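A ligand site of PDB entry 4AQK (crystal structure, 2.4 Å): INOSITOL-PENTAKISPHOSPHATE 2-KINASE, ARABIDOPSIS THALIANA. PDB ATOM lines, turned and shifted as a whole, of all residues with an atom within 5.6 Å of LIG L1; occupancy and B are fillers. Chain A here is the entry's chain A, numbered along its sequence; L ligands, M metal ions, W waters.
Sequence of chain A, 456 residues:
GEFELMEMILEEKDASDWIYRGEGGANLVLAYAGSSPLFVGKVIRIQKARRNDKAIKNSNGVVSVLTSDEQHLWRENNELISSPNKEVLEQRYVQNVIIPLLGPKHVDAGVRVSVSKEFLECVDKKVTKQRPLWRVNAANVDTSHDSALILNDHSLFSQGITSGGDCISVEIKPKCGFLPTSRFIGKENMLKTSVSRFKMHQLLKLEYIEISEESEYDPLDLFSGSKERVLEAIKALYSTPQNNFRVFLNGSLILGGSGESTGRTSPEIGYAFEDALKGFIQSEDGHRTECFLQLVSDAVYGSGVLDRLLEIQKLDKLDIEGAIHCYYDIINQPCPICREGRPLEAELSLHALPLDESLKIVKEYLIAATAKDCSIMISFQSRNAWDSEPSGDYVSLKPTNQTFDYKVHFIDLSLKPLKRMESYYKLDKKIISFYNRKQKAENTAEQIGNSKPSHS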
ATOM      1  N   GLU A  23     -13.349  -4.849  -8.849  1.00  0.00           N
ATOM      2  CA  GLU A  23     -12.550  -4.160  -7.842  1.00  0.00           C
ATOM      3  C   GLU A  23     -12.647  -2.653  -7.992  1.00  0.00           C
ATOM      4  O   GLU A  23     -13.024  -2.135  -9.051  1.00  0.00           O
ATOM      5  CB  GLU A  23     -11.079  -4.600  -7.898  1.00  0.00           C
ATOM      6  CG  GLU A  23     -10.309  -4.167  -9.131  1.00  0.00           C
ATOM      7  CD  GLU A  23      -8.900  -4.705  -9.137  1.00  0.00           C
ATOM      8  OE1 GLU A  23      -8.058  -4.199  -8.375  1.00  0.00           O
ATOM      9  OE2 GLU A  23      -8.626  -5.660  -9.879  1.00  0.00           O
ATOM     10  N   GLY A  24     -12.322  -1.946  -6.915  1.00  0.00           N
ATOM     11  CA  GLY A  24     -12.107  -0.504  -6.963  1.00  0.00           C
ATOM     12  C   GLY A  24     -10.640  -0.239  -6.691  1.00  0.00           C
ATOM     13  O   GLY A  24      -9.773  -0.915  -7.235  1.00  0.00           O
ATOM     14  N   GLY A  25     -10.375   0.737  -5.829  1.00  0.00           N
ATOM     15  CA  GLY A  25      -9.002   1.104  -5.503  1.00  0.00           C
ATOM     16  C   GLY A  25      -8.500   0.498  -4.198  1.00  0.00           C
ATOM     17  O   GLY A  25      -7.287   0.330  -4.023  1.00  0.00           O
ATOM     18  N   ALA A  26      -9.410   0.176  -3.297  1.00  0.00           N
ATOM     19  CA  ALA A  26      -9.044  -0.349  -1.982  1.00  0.00           C
ATOM     20  C   ALA A  26      -9.361  -1.831  -1.794  1.00  0.00           C
ATOM     21  O   ALA A  26      -8.741  -2.502  -0.967  1.00  0.00           O
ATOM     22  CB  ALA A  26      -9.714   0.479  -0.883  1.00  0.00           C
ATOM     23  N   ARG A  50      -1.154  -1.119  -1.742  1.00  0.00           N
ATOM     24  CA  ARG A  50      -0.321  -0.577  -2.820  1.00  0.00           C
ATOM     25  C   ARG A  50       1.053  -1.241  -2.818  1.00  0.00           C
ATOM     26  O   ARG A  50       1.463  -1.834  -1.820  1.00  0.00           O
ATOM     27  CB  ARG A  50      -0.214   0.940  -2.734  1.00  0.00           C
ATOM     28  CG  ARG A  50      -1.352   1.642  -3.442  1.00  0.00           C
ATOM     29  CD  ARG A  50      -1.941   2.756  -2.582  1.00  0.00           C
ATOM     30  NE  ARG A  50      -3.393   2.620  -2.501  1.00  0.00           N
ATOM     31  CZ  ARG A  50      -4.200   3.410  -1.810  1.00  0.00           C
ATOM     32  NH1 ARG A  50      -3.709   4.446  -1.129  1.00  0.00           N
ATOM     33  NH2 ARG A  50      -5.504   3.181  -1.804  1.00  0.00           N
ATOM     34  N   TRP A 134      -3.445  -2.101 -15.389  1.00  0.00           N
ATOM     35  CA  TRP A 134      -3.064  -0.974 -14.543  1.00  0.00           C
ATOM     36  C   TRP A 134      -3.416  -1.177 -13.071  1.00  0.00           C
ATOM     37  O   TRP A 134      -2.696  -0.703 -12.195  1.00  0.00           O
ATOM     38  CB  TRP A 134      -3.639   0.333 -15.072  1.00  0.00           C
ATOM     39  CG  TRP A 134      -5.138   0.425 -15.049  1.00  0.00           C
ATOM     40  CD1 TRP A 134      -6.005   0.033 -16.024  1.00  0.00           C
ATOM     41  CD2 TRP A 134      -5.935   0.997 -14.010  1.00  0.00           C
ATOM     42  NE1 TRP A 134      -7.299   0.309 -15.656  1.00  0.00           N
ATOM     43  CE2 TRP A 134      -7.285   0.894 -14.416  1.00  0.00           C
ATOM     44  CE3 TRP A 134      -5.645   1.580 -12.766  1.00  0.00           C
ATOM     45  CZ2 TRP A 134      -8.340   1.360 -13.631  1.00  0.00           C
ATOM     46  CZ3 TRP A 134      -6.703   2.035 -11.974  1.00  0.00           C
ATOM     47  CH2 TRP A 134      -8.033   1.927 -12.410  1.00  0.00           C
ATOM     48  N   ARG A 135      -4.514  -1.897 -12.811  1.00  0.00           N
ATOM     49  CA  ARG A 135      -4.868  -2.318 -11.456  1.00  0.00           C
ATOM     50  C   ARG A 135      -3.773  -3.194 -10.847  1.00  0.00           C
ATOM     51  O   ARG A 135      -3.373  -2.975  -9.708  1.00  0.00           O
ATOM     52  CB  ARG A 135      -6.197  -3.087 -11.454  1.00  0.00           C
ATOM     53  CG  ARG A 135      -7.445  -2.233 -11.625  1.00  0.00           C
ATOM     54  CD  ARG A 135      -7.591  -1.163 -10.552  1.00  0.00           C
ATOM     55  NE  ARG A 135      -8.965  -0.685 -10.457  1.00  0.00           N
ATOM     56  CZ  ARG A 135      -9.360   0.410  -9.816  1.00  0.00           C
ATOM     57  NH1 ARG A 135      -8.481   1.187  -9.190  1.00  0.00           N
ATOM     58  NH2 ARG A 135     -10.643   0.736  -9.808  1.00  0.00           N
ATOM     59  N   LYS A 173     -22.384   4.532  -9.571  1.00  0.00           N
ATOM     60  CA  LYS A 173     -21.450   5.330  -8.759  1.00  0.00           C
ATOM     61  C   LYS A 173     -21.747   6.800  -9.024  1.00  0.00           C
ATOM     62  O   LYS A 173     -21.268   7.385 -10.004  1.00  0.00           O
ATOM     63  CB  LYS A 173     -20.009   5.010  -9.123  1.00  0.00           C
ATOM     64  CG  LYS A 173     -19.007   5.311  -8.040  1.00  0.00           C
ATOM     65  CD  LYS A 173     -17.604   5.318  -8.611  1.00  0.00           C
ATOM     66  CE  LYS A 173     -16.617   4.644  -7.679  1.00  0.00           C
ATOM     67  NZ  LYS A 173     -16.268   5.507  -6.528  1.00  0.00           N
ATOM     68  N   LYS A 175     -21.091   9.718  -7.601  1.00  0.00           N
ATOM     69  CA  LYS A 175     -20.125  10.782  -7.315  1.00  0.00           C
ATOM     70  C   LYS A 175     -20.775  11.943  -6.566  1.00  0.00           C
ATOM     71  O   LYS A 175     -21.858  11.796  -5.983  1.00  0.00           O
ATOM     72  CB  LYS A 175     -19.394  11.254  -8.600  1.00  0.00           C
ATOM     73  CG  LYS A 175     -18.401  10.251  -9.203  1.00  0.00           C
ATOM     74  CD  LYS A 175     -17.581   9.484  -8.140  1.00  0.00           C
ATOM     75  CE  LYS A 175     -16.433  10.307  -7.577  1.00  0.00           C
ATOM     76  NZ  LYS A 175     -15.435   9.433  -6.890  1.00  0.00           N
ATOM     77  N   ARG A 197     -17.370  19.094  -9.832  1.00  0.00           N
ATOM     78  CA  ARG A 197     -16.126  18.398  -9.736  1.00  0.00           C
ATOM     79  C   ARG A 197     -16.042  17.255 -10.761  1.00  0.00           C
ATOM     80  O   ARG A 197     -15.014  17.081 -11.413  1.00  0.00           O
ATOM     81  CB  ARG A 197     -15.945  17.856  -8.309  1.00  0.00           C
ATOM     82  CG  ARG A 197     -15.061  16.650  -8.195  1.00  0.00           C
ATOM     83  CD  ARG A 197     -13.608  16.981  -8.492  1.00  0.00           C
ATOM     84  NE  ARG A 197     -12.729  16.269  -7.575  1.00  0.00           N
ATOM     85  CZ  ARG A 197     -12.058  16.839  -6.591  1.00  0.00           C
ATOM     86  NH1 ARG A 197     -12.120  18.141  -6.404  1.00  0.00           N
ATOM     87  NH2 ARG A 197     -11.298  16.091  -5.795  1.00  0.00           N
ATOM     88  N   HIS A 201     -12.967  16.842 -13.326  1.00  0.00           N
ATOM     89  CA  HIS A 201     -12.031  15.730 -13.228  1.00  0.00           C
ATOM     90  C   HIS A 201     -11.874  14.999 -14.570  1.00  0.00           C
ATOM     91  O   HIS A 201     -10.798  14.505 -14.894  1.00  0.00           O
ATOM     92  CB  HIS A 201     -12.448  14.768 -12.126  1.00  0.00           C
ATOM     93  CG  HIS A 201     -11.300  14.037 -11.500  1.00  0.00           C
ATOM     94  ND1 HIS A 201     -11.381  13.444 -10.258  1.00  0.00           N
ATOM     95  CD2 HIS A 201     -10.034  13.832 -11.930  1.00  0.00           C
ATOM     96  CE1 HIS A 201     -10.224  12.898  -9.955  1.00  0.00           C
ATOM     97  NE2 HIS A 201      -9.380  13.119 -10.951  1.00  0.00           N
ATOM     98  N   LYS A 205      -8.434  13.468 -16.233  1.00  0.00           N
ATOM     99  CA  LYS A 205      -8.392  12.034 -16.506  1.00  0.00           C
ATOM    100  C   LYS A 205      -8.062  11.738 -17.966  1.00  0.00           C
ATOM    101  O   LYS A 205      -7.236  10.867 -18.251  1.00  0.00           O
ATOM    102  CB  LYS A 205      -9.716  11.383 -16.132  1.00  0.00           C
ATOM    103  CG  LYS A 205      -9.981  11.218 -14.641  1.00  0.00           C
ATOM    104  CD  LYS A 205     -11.380  10.657 -14.455  1.00  0.00           C
ATOM    105  CE  LYS A 205     -11.845  10.730 -13.028  1.00  0.00           C
ATOM    106  NZ  LYS A 205     -11.429   9.524 -12.264  1.00  0.00           N
ATOM    107  N   ASN A 243     -16.686   4.323 -15.112  1.00  0.00           N
ATOM    108  CA  ASN A 243     -16.766   3.501 -13.914  1.00  0.00           C
ATOM    109  C   ASN A 243     -18.002   3.788 -13.043  1.00  0.00           C
ATOM    110  O   ASN A 243     -18.070   3.369 -11.884  1.00  0.00           O
ATOM    111  CB  ASN A 243     -15.455   3.513 -13.115  1.00  0.00           C
ATOM    112  CG  ASN A 243     -15.137   4.857 -12.462  1.00  0.00           C
ATOM    113  OD1 ASN A 243     -14.341   4.916 -11.526  1.00  0.00           O
ATOM    114  ND2 ASN A 243     -15.744   5.943 -12.956  1.00  0.00           N
ATOM    115  N   ASN A 244     -18.994   4.460 -13.629  1.00  0.00           N
ATOM    116  CA  ASN A 244     -20.151   4.913 -12.871  1.00  0.00           C
ATOM    117  C   ASN A 244     -21.421   4.120 -13.116  1.00  0.00           C
ATOM    118  O   ASN A 244     -22.441   4.339 -12.467  1.00  0.00           O
ATOM    119  CB  ASN A 244     -20.418   6.404 -13.146  1.00  0.00           C
ATOM    120  CG  ASN A 244     -19.194   7.261 -12.941  1.00  0.00           C
ATOM    121  OD1 ASN A 244     -18.484   7.564 -13.895  1.00  0.00           O
ATOM    122  ND2 ASN A 244     -18.916   7.620 -11.692  1.00  0.00           N
ATOM    123  N   ALA A 369     -16.829  12.393   2.159  1.00  0.00           N
ATOM    124  CA  ALA A 369     -15.988  11.736   1.151  1.00  0.00           C
ATOM    125  C   ALA A 369     -16.333  10.254   0.945  1.00  0.00           C
ATOM    126  O   ALA A 369     -16.211   9.727  -0.156  1.00  0.00           O
ATOM    127  CB  ALA A 369     -14.498  11.901   1.508  1.00  0.00           C
ATOM    128  N   ASP A 373     -18.056   8.730  -2.751  1.00  0.00           N
ATOM    129  CA  ASP A 373     -17.320   7.639  -3.378  1.00  0.00           C
ATOM    130  C   ASP A 373     -17.987   6.254  -3.280  1.00  0.00           C
ATOM    131  O   ASP A 373     -17.422   5.246  -3.710  1.00  0.00           O
ATOM    132  CB  ASP A 373     -15.911   7.583  -2.797  1.00  0.00           C
ATOM    133  CG  ASP A 373     -14.970   6.734  -3.611  1.00  0.00           C
ATOM    134  OD1 ASP A 373     -14.847   7.005  -4.834  1.00  0.00           O
ATOM    135  OD2 ASP A 373     -14.341   5.817  -3.037  1.00  0.00           O
ATOM    136  N   ASP A 412     -19.606  -0.234  -0.988  1.00  0.00           N
ATOM    137  CA  ASP A 412     -18.358   0.517  -1.046  1.00  0.00           C
ATOM    138  C   ASP A 412     -18.424   1.739  -0.125  1.00  0.00           C
ATOM    139  O   ASP A 412     -18.277   2.879  -0.567  1.00  0.00           O
ATOM    140  CB  ASP A 412     -18.061   0.927  -2.494  1.00  0.00           C
ATOM    141  CG  ASP A 412     -16.732   1.648  -2.661  1.00  0.00           C
ATOM    142  OD1 ASP A 412     -15.834   1.474  -1.805  1.00  0.00           O
ATOM    143  OD2 ASP A 412     -16.591   2.376  -3.669  1.00  0.00           O
ATOM    144  N   SER A 414     -16.325   2.818   2.358  1.00  0.00           N
ATOM    145  CA  SER A 414     -15.012   2.754   3.002  1.00  0.00           C
ATOM    146  C   SER A 414     -14.697   3.948   3.924  1.00  0.00           C
ATOM    147  O   SER A 414     -15.051   5.090   3.619  1.00  0.00           O
ATOM    148  CB  SER A 414     -13.900   2.622   1.947  1.00  0.00           C
ATOM    149  OG  SER A 414     -14.164   1.560   1.047  1.00  0.00           O
ATOM    150  N   LYS A 416     -12.300   6.668   5.013  1.00  0.00           N
ATOM    151  CA  LYS A 416     -11.217   7.422   4.382  1.00  0.00           C
ATOM    152  C   LYS A 416     -10.168   7.800   5.432  1.00  0.00           C
ATOM    153  O   LYS A 416     -10.533   8.263   6.515  1.00  0.00           O
ATOM    154  CB  LYS A 416     -11.754   8.672   3.675  1.00  0.00           C
ATOM    155  CG  LYS A 416     -12.890   8.409   2.706  1.00  0.00           C
ATOM    156  CD  LYS A 416     -12.448   7.609   1.492  1.00  0.00           C
ATOM    157  CE  LYS A 416     -13.643   7.092   0.727  1.00  0.00           C
ATOM    158  NZ  LYS A 416     -13.230   6.361  -0.494  1.00  0.00           N
ATOM    159  N   ARG A 420      -5.136  11.651   4.154  1.00  0.00           N
ATOM    160  CA  ARG A 420      -5.558  11.905   2.768  1.00  0.00           C
ATOM    161  C   ARG A 420      -6.069  13.324   2.507  1.00  0.00           C
ATOM    162  O   ARG A 420      -6.234  13.727   1.350  1.00  0.00           O
ATOM    163  CB  ARG A 420      -6.613  10.873   2.350  1.00  0.00           C
ATOM    164  CG  ARG A 420      -6.701  10.642   0.846  1.00  0.00           C
ATOM    165  CD  ARG A 420      -7.666   9.515   0.522  1.00  0.00           C
ATOM    166  NE  ARG A 420      -7.021   8.198   0.485  1.00  0.00           N
ATOM    167  CZ  ARG A 420      -7.637   7.075   0.161  1.00  0.00           C
ATOM    168  NH1 ARG A 420      -8.930   7.076  -0.146  1.00  0.00           N
ATOM    169  NH2 ARG A 420      -6.969   5.929   0.150  1.00  0.00           N
ATOM    170  N   TYR A 424      -6.091  15.195  -1.108  1.00  0.00           N
ATOM    171  CA  TYR A 424      -7.341  15.798  -1.577  1.00  0.00           C
ATOM    172  C   TYR A 424      -7.116  17.232  -2.032  1.00  0.00           C
ATOM    173  O   TYR A 424      -7.499  17.611  -3.139  1.00  0.00           O
ATOM    174  CB  TYR A 424      -8.420  15.759  -0.504  1.00  0.00           C
ATOM    175  CG  TYR A 424      -9.034  14.399  -0.229  1.00  0.00           C
ATOM    176  CD1 TYR A 424      -9.180  13.446  -1.253  1.00  0.00           C
ATOM    177  CD2 TYR A 424      -9.479  14.057   1.048  1.00  0.00           C
ATOM    178  CE1 TYR A 424      -9.737  12.204  -1.008  1.00  0.00           C
ATOM    179  CE2 TYR A 424     -10.053  12.823   1.301  1.00  0.00           C
ATOM    180  CZ  TYR A 424     -10.184  11.895   0.284  1.00  0.00           C
ATOM    181  OH  TYR A 424     -10.742  10.661   0.545  1.00  0.00           O
ATOM    182  N   LEU A 427      -4.926  17.329  -5.223  1.00  0.00           N
ATOM    183  CA  LEU A 427      -5.695  16.882  -6.377  1.00  0.00           C
ATOM    184  C   LEU A 427      -6.687  17.958  -6.811  1.00  0.00           C
ATOM    185  O   LEU A 427      -6.807  18.255  -7.991  1.00  0.00           O
ATOM    186  CB  LEU A 427      -6.417  15.561  -6.094  1.00  0.00           C
ATOM    187  CG  LEU A 427      -7.153  14.881  -7.267  1.00  0.00           C
ATOM    188  CD1 LEU A 427      -6.206  14.452  -8.368  1.00  0.00           C
ATOM    189  CD2 LEU A 427      -7.988  13.694  -6.790  1.00  0.00           C
HETATM  190  C1  LIG L   1     -11.492   7.522  -4.759  1.00  0.00           C
HETATM  191  C2  LIG L   1     -10.787   6.167  -4.836  1.00  0.00           C
HETATM  192  C3  LIG L   1     -11.354   5.278  -5.937  1.00  0.00           C
HETATM  193  C4  LIG L   1     -11.321   6.015  -7.284  1.00  0.00           C
HETATM  194  C5  LIG L   1     -12.050   7.369  -7.235  1.00  0.00           C
HETATM  195  C6  LIG L   1     -11.526   8.262  -6.100  1.00  0.00           C
HETATM  196  O1  LIG L   1     -10.819   8.340  -3.801  1.00  0.00           O
HETATM  197  P1  LIG L   1     -11.555   9.084  -2.567  1.00  0.00           P
HETATM  198  O2  LIG L   1     -11.747  10.485  -3.064  1.00  0.00           O
HETATM  199  O3  LIG L   1     -12.837   8.358  -2.313  1.00  0.00           O
HETATM  200  O4  LIG L   1     -10.565   8.917  -1.428  1.00  0.00           O
HETATM  201  O5  LIG L   1     -10.975   5.517  -3.584  1.00  0.00           O
HETATM  202  P2  LIG L   1      -9.823   4.694  -2.820  1.00  0.00           P
HETATM  203  O6  LIG L   1     -10.016   3.274  -3.267  1.00  0.00           O
HETATM  204  O7  LIG L   1      -8.493   5.262  -3.254  1.00  0.00           O
HETATM  205  O8  LIG L   1     -10.197   4.936  -1.374  1.00  0.00           O
HETATM  206  O9  LIG L   1     -12.683   4.871  -5.601  1.00  0.00           O
HETATM  207  P3  LIG L   1     -13.094   3.348  -5.198  1.00  0.00           P
HETATM  208  O10 LIG L   1     -13.614   2.754  -6.494  1.00  0.00           O
HETATM  209  O11 LIG L   1     -11.851   2.693  -4.661  1.00  0.00           O
HETATM  210  O12 LIG L   1     -14.158   3.473  -4.135  1.00  0.00           O
HETATM  211  O13 LIG L   1     -11.896   5.201  -8.296  1.00  0.00           O
HETATM  212  P4  LIG L   1     -11.061   4.310  -9.359  1.00  0.00           P
HETATM  213  O14 LIG L   1      -9.951   3.651  -8.571  1.00  0.00           O
HETATM  214  O15 LIG L   1     -10.571   5.270 -10.402  1.00  0.00           O
HETATM  215  O16 LIG L   1     -12.132   3.375  -9.866  1.00  0.00           O
HETATM  216  O17 LIG L   1     -11.877   8.048  -8.472  1.00  0.00           O
HETATM  217  P5  LIG L   1     -12.986   8.210  -9.631  1.00  0.00           P
HETATM  218  O18 LIG L   1     -12.894   9.648 -10.065  1.00  0.00           O
HETATM  219  O19 LIG L   1     -12.523   7.246 -10.697  1.00  0.00           O
HETATM  220  O20 LIG L   1     -14.318   7.899  -8.996  1.00  0.00           O
HETATM  221  O21 LIG L   1     -12.377   9.392  -5.942  1.00  0.00           O
HETATM  222  P6  LIG L   1     -11.996  10.893  -6.414  1.00  0.00           P
HETATM  223  O22 LIG L   1     -13.303  11.639  -6.464  1.00  0.00           O
HETATM  224  O23 LIG L   1     -11.086  11.329  -5.309  1.00  0.00           O
HETATM  225  O24 LIG L   1     -11.358  10.758  -7.786  1.00  0.00           O
HETATM  226  P1  LG2 L   2     -13.413  -0.815  -3.531  1.00  0.00           P
HETATM  227  O1  LG2 L   2     -12.026  -1.214  -3.962  1.00  0.00           O
HETATM  228  O2  LG2 L   2     -13.949   0.369  -4.300  1.00  0.00           O
HETATM  229  O3  LG2 L   2     -13.572  -0.722  -2.031  1.00  0.00           O
HETATM  230  P2  LG2 L   2     -15.995  -1.989  -3.977  1.00  0.00           P
HETATM  231  O4  LG2 L   2     -16.480  -2.235  -2.571  1.00  0.00           O
HETATM  232  O5  LG2 L   2     -16.460  -0.768  -4.735  1.00  0.00           O
HETATM  233  O6  LG2 L   2     -14.368  -2.050  -3.960  1.00  0.00           O
HETATM  234  O7  LG2 L   2     -16.369  -3.273  -4.881  1.00  0.00           O
HETATM  235  C1  LG2 L   2     -15.794  -3.468  -6.164  1.00  0.00           C
HETATM  236  C2  LG2 L   2     -16.814  -3.932  -7.190  1.00  0.00           C
HETATM  237  O8  LG2 L   2     -17.398  -5.192  -6.823  1.00  0.00           O
HETATM  238  C3  LG2 L   2     -17.959  -2.945  -7.328  1.00  0.00           C
HETATM  239  O9  LG2 L   2     -17.778  -2.126  -8.483  1.00  0.00           O
HETATM  240  C4  LG2 L   2     -19.228  -3.789  -7.405  1.00  0.00           C
HETATM  241  O10 LG2 L   2     -19.713  -3.910  -8.738  1.00  0.00           O
HETATM  242  C5  LG2 L   2     -18.828  -5.167  -6.923  1.00  0.00           C
HETATM  243  N1  LG2 L   2     -19.452  -5.449  -5.602  1.00  0.00           N
HETATM  244  C6  LG2 L   2     -18.974  -5.078  -4.403  1.00  0.00           C
HETATM  245  N2  LG2 L   2     -19.766  -5.506  -3.386  1.00  0.00           N
HETATM  246  C7  LG2 L   2     -20.788  -6.181  -3.935  1.00  0.00           C
HETATM  247  C8  LG2 L   2     -21.989  -6.905  -3.442  1.00  0.00           C
HETATM  248  N3  LG2 L   2     -22.275  -6.984  -2.121  1.00  0.00           N
HETATM  249  N4  LG2 L   2     -22.805  -7.467  -4.357  1.00  0.00           N
HETATM  250  C9  LG2 L   2     -22.554  -7.401  -5.687  1.00  0.00           C
HETATM  251  N5  LG2 L   2     -21.487  -6.756  -6.206  1.00  0.00           N
HETATM  252  C10 LG2 L   2     -20.577  -6.147  -5.404  1.00  0.00           C
HETATM  253 MG    MG M   1     -13.314   2.346  -1.520  1.00  0.00          MG
HETATM  254  O   HOH W   1     -11.338   3.529 -13.172  1.00  0.00           O
HETATM  255  O   HOH W   2     -15.957   0.609  -6.813  1.00  0.00           O
HETATM  256  O   HOH W   3      -7.799   9.425  -3.103  1.00  0.00           O
HETATM  257  O   HOH W   4     -16.056   8.121 -11.310  1.00  0.00           O
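NH1 of Arg 135 lies close to O of Gly 24. OD1 of Asp 412 sits at hydrogen-bond distance from OG of Ser 414 (3.3 Å). N of Lys 173 lies within hydrogen-bond range of O of Asn 244, at 2.9 Å. OD1 of Asn 244 lies within hydrogen-bond range of ND2 of Asn 243, at 3.3 Å. OD1 of Asp 373 is in salt-bridge range of NZ of Lys 175 (3.2 Å). The side-chain carboxylate (OD2) of Asp 373 is in salt-bridge range of the side-chain amino group (NZ) of Lys 416, at 2.8 Å. The side-chain carboxylate (OD1) of Asp 373 lies within salt-bridge range of the side-chain amino group (NZ) of Lys 173, 2.7 Å away.
An oxygen (O6) of LIG L1 lies within hydrogen-bond range of the backbone NH (N) of Ala 26, at 3.2 Å. The side-chain hydroxyl (OH) of Tyr 424 sits at hydrogen-bond distance from an oxygen (O4) of LIG L1 (2.6 Å). The backbone NH (N) of Gly 25 sits at hydrogen-bond distance from an oxygen (O11) of LIG L1, 2.7 Å away. The side-chain amino group of Lys 416 lies within salt-bridge range of an oxygen (O3) of LIG L1 (2.7 Å). The backbone NH (N) of Gly 24 sits at hydrogen-bond distance from an oxygen (O1) of LG2 L2, at 3.1 Å. An oxygen (O12) of LIG L1 sits close to the side-chain carboxylate (OD2) of Asp 412, 2.7 Å away. O12 of LIG L1 lies within salt-bridge range of NZ of Lys 173, 3.8 Å away. N of Gly 25 sits at hydrogen-bond distance from O1 of LG2 L2, 3.2 Å away. OD2 of Asp 373 lies close to O12 of LIG L1, at 2.6 Å. NH1 of Arg 420 lies within salt-bridge range of O8 of LIG L1 (2.8 Å). An oxygen (O19) of LIG L1 lies close to the side-chain amide oxygen (OD1) of Asn 243 (3.1 Å). The side-chain amino group (NZ) of Lys 175 is in salt-bridge range of an oxygen (O20) of LIG L1. An oxygen (O7) of LIG L1 lies within salt-bridge range of the guanidinium group of Arg 50 (3.9 Å). An oxygen (O1) of LG2 L2 is in hydrogen-bond range of the backbone NH (N) of Ala 26. The side-chain amino group of Lys 205 is in salt-bridge range of an oxygen (O18) of LIG L1, at 2.6 Å. NH1 of Arg 135 lies within salt-bridge range of O14 of LIG L1.
CA of Gly 24 touches O10 of LIG L1, 3.6 Å away. His 201 touches LIG L1 (CE1 to O24, 3.3 Å). Within 4 Å of LIG L1: Gly 24, Gly 25, Ala 26, Arg 50, Arg 135, Lys 173, Lys 175, His 201, Lys 205, Asn 243, Asp 373, Asp 412, Lys 416, Arg 420 and Tyr 424.
Water W4 lies within hydrogen-bond range of the side-chain amide nitrogen (ND2) of Asn 243 (2.7 Å), an oxygen (O20) of LIG L1 (2.9 Å) and the side-chain amide nitrogen (ND2) of Asn 244 (2.9 Å). Water W2 bridges O5 of LG2 L2 and O10 of LIG L1.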
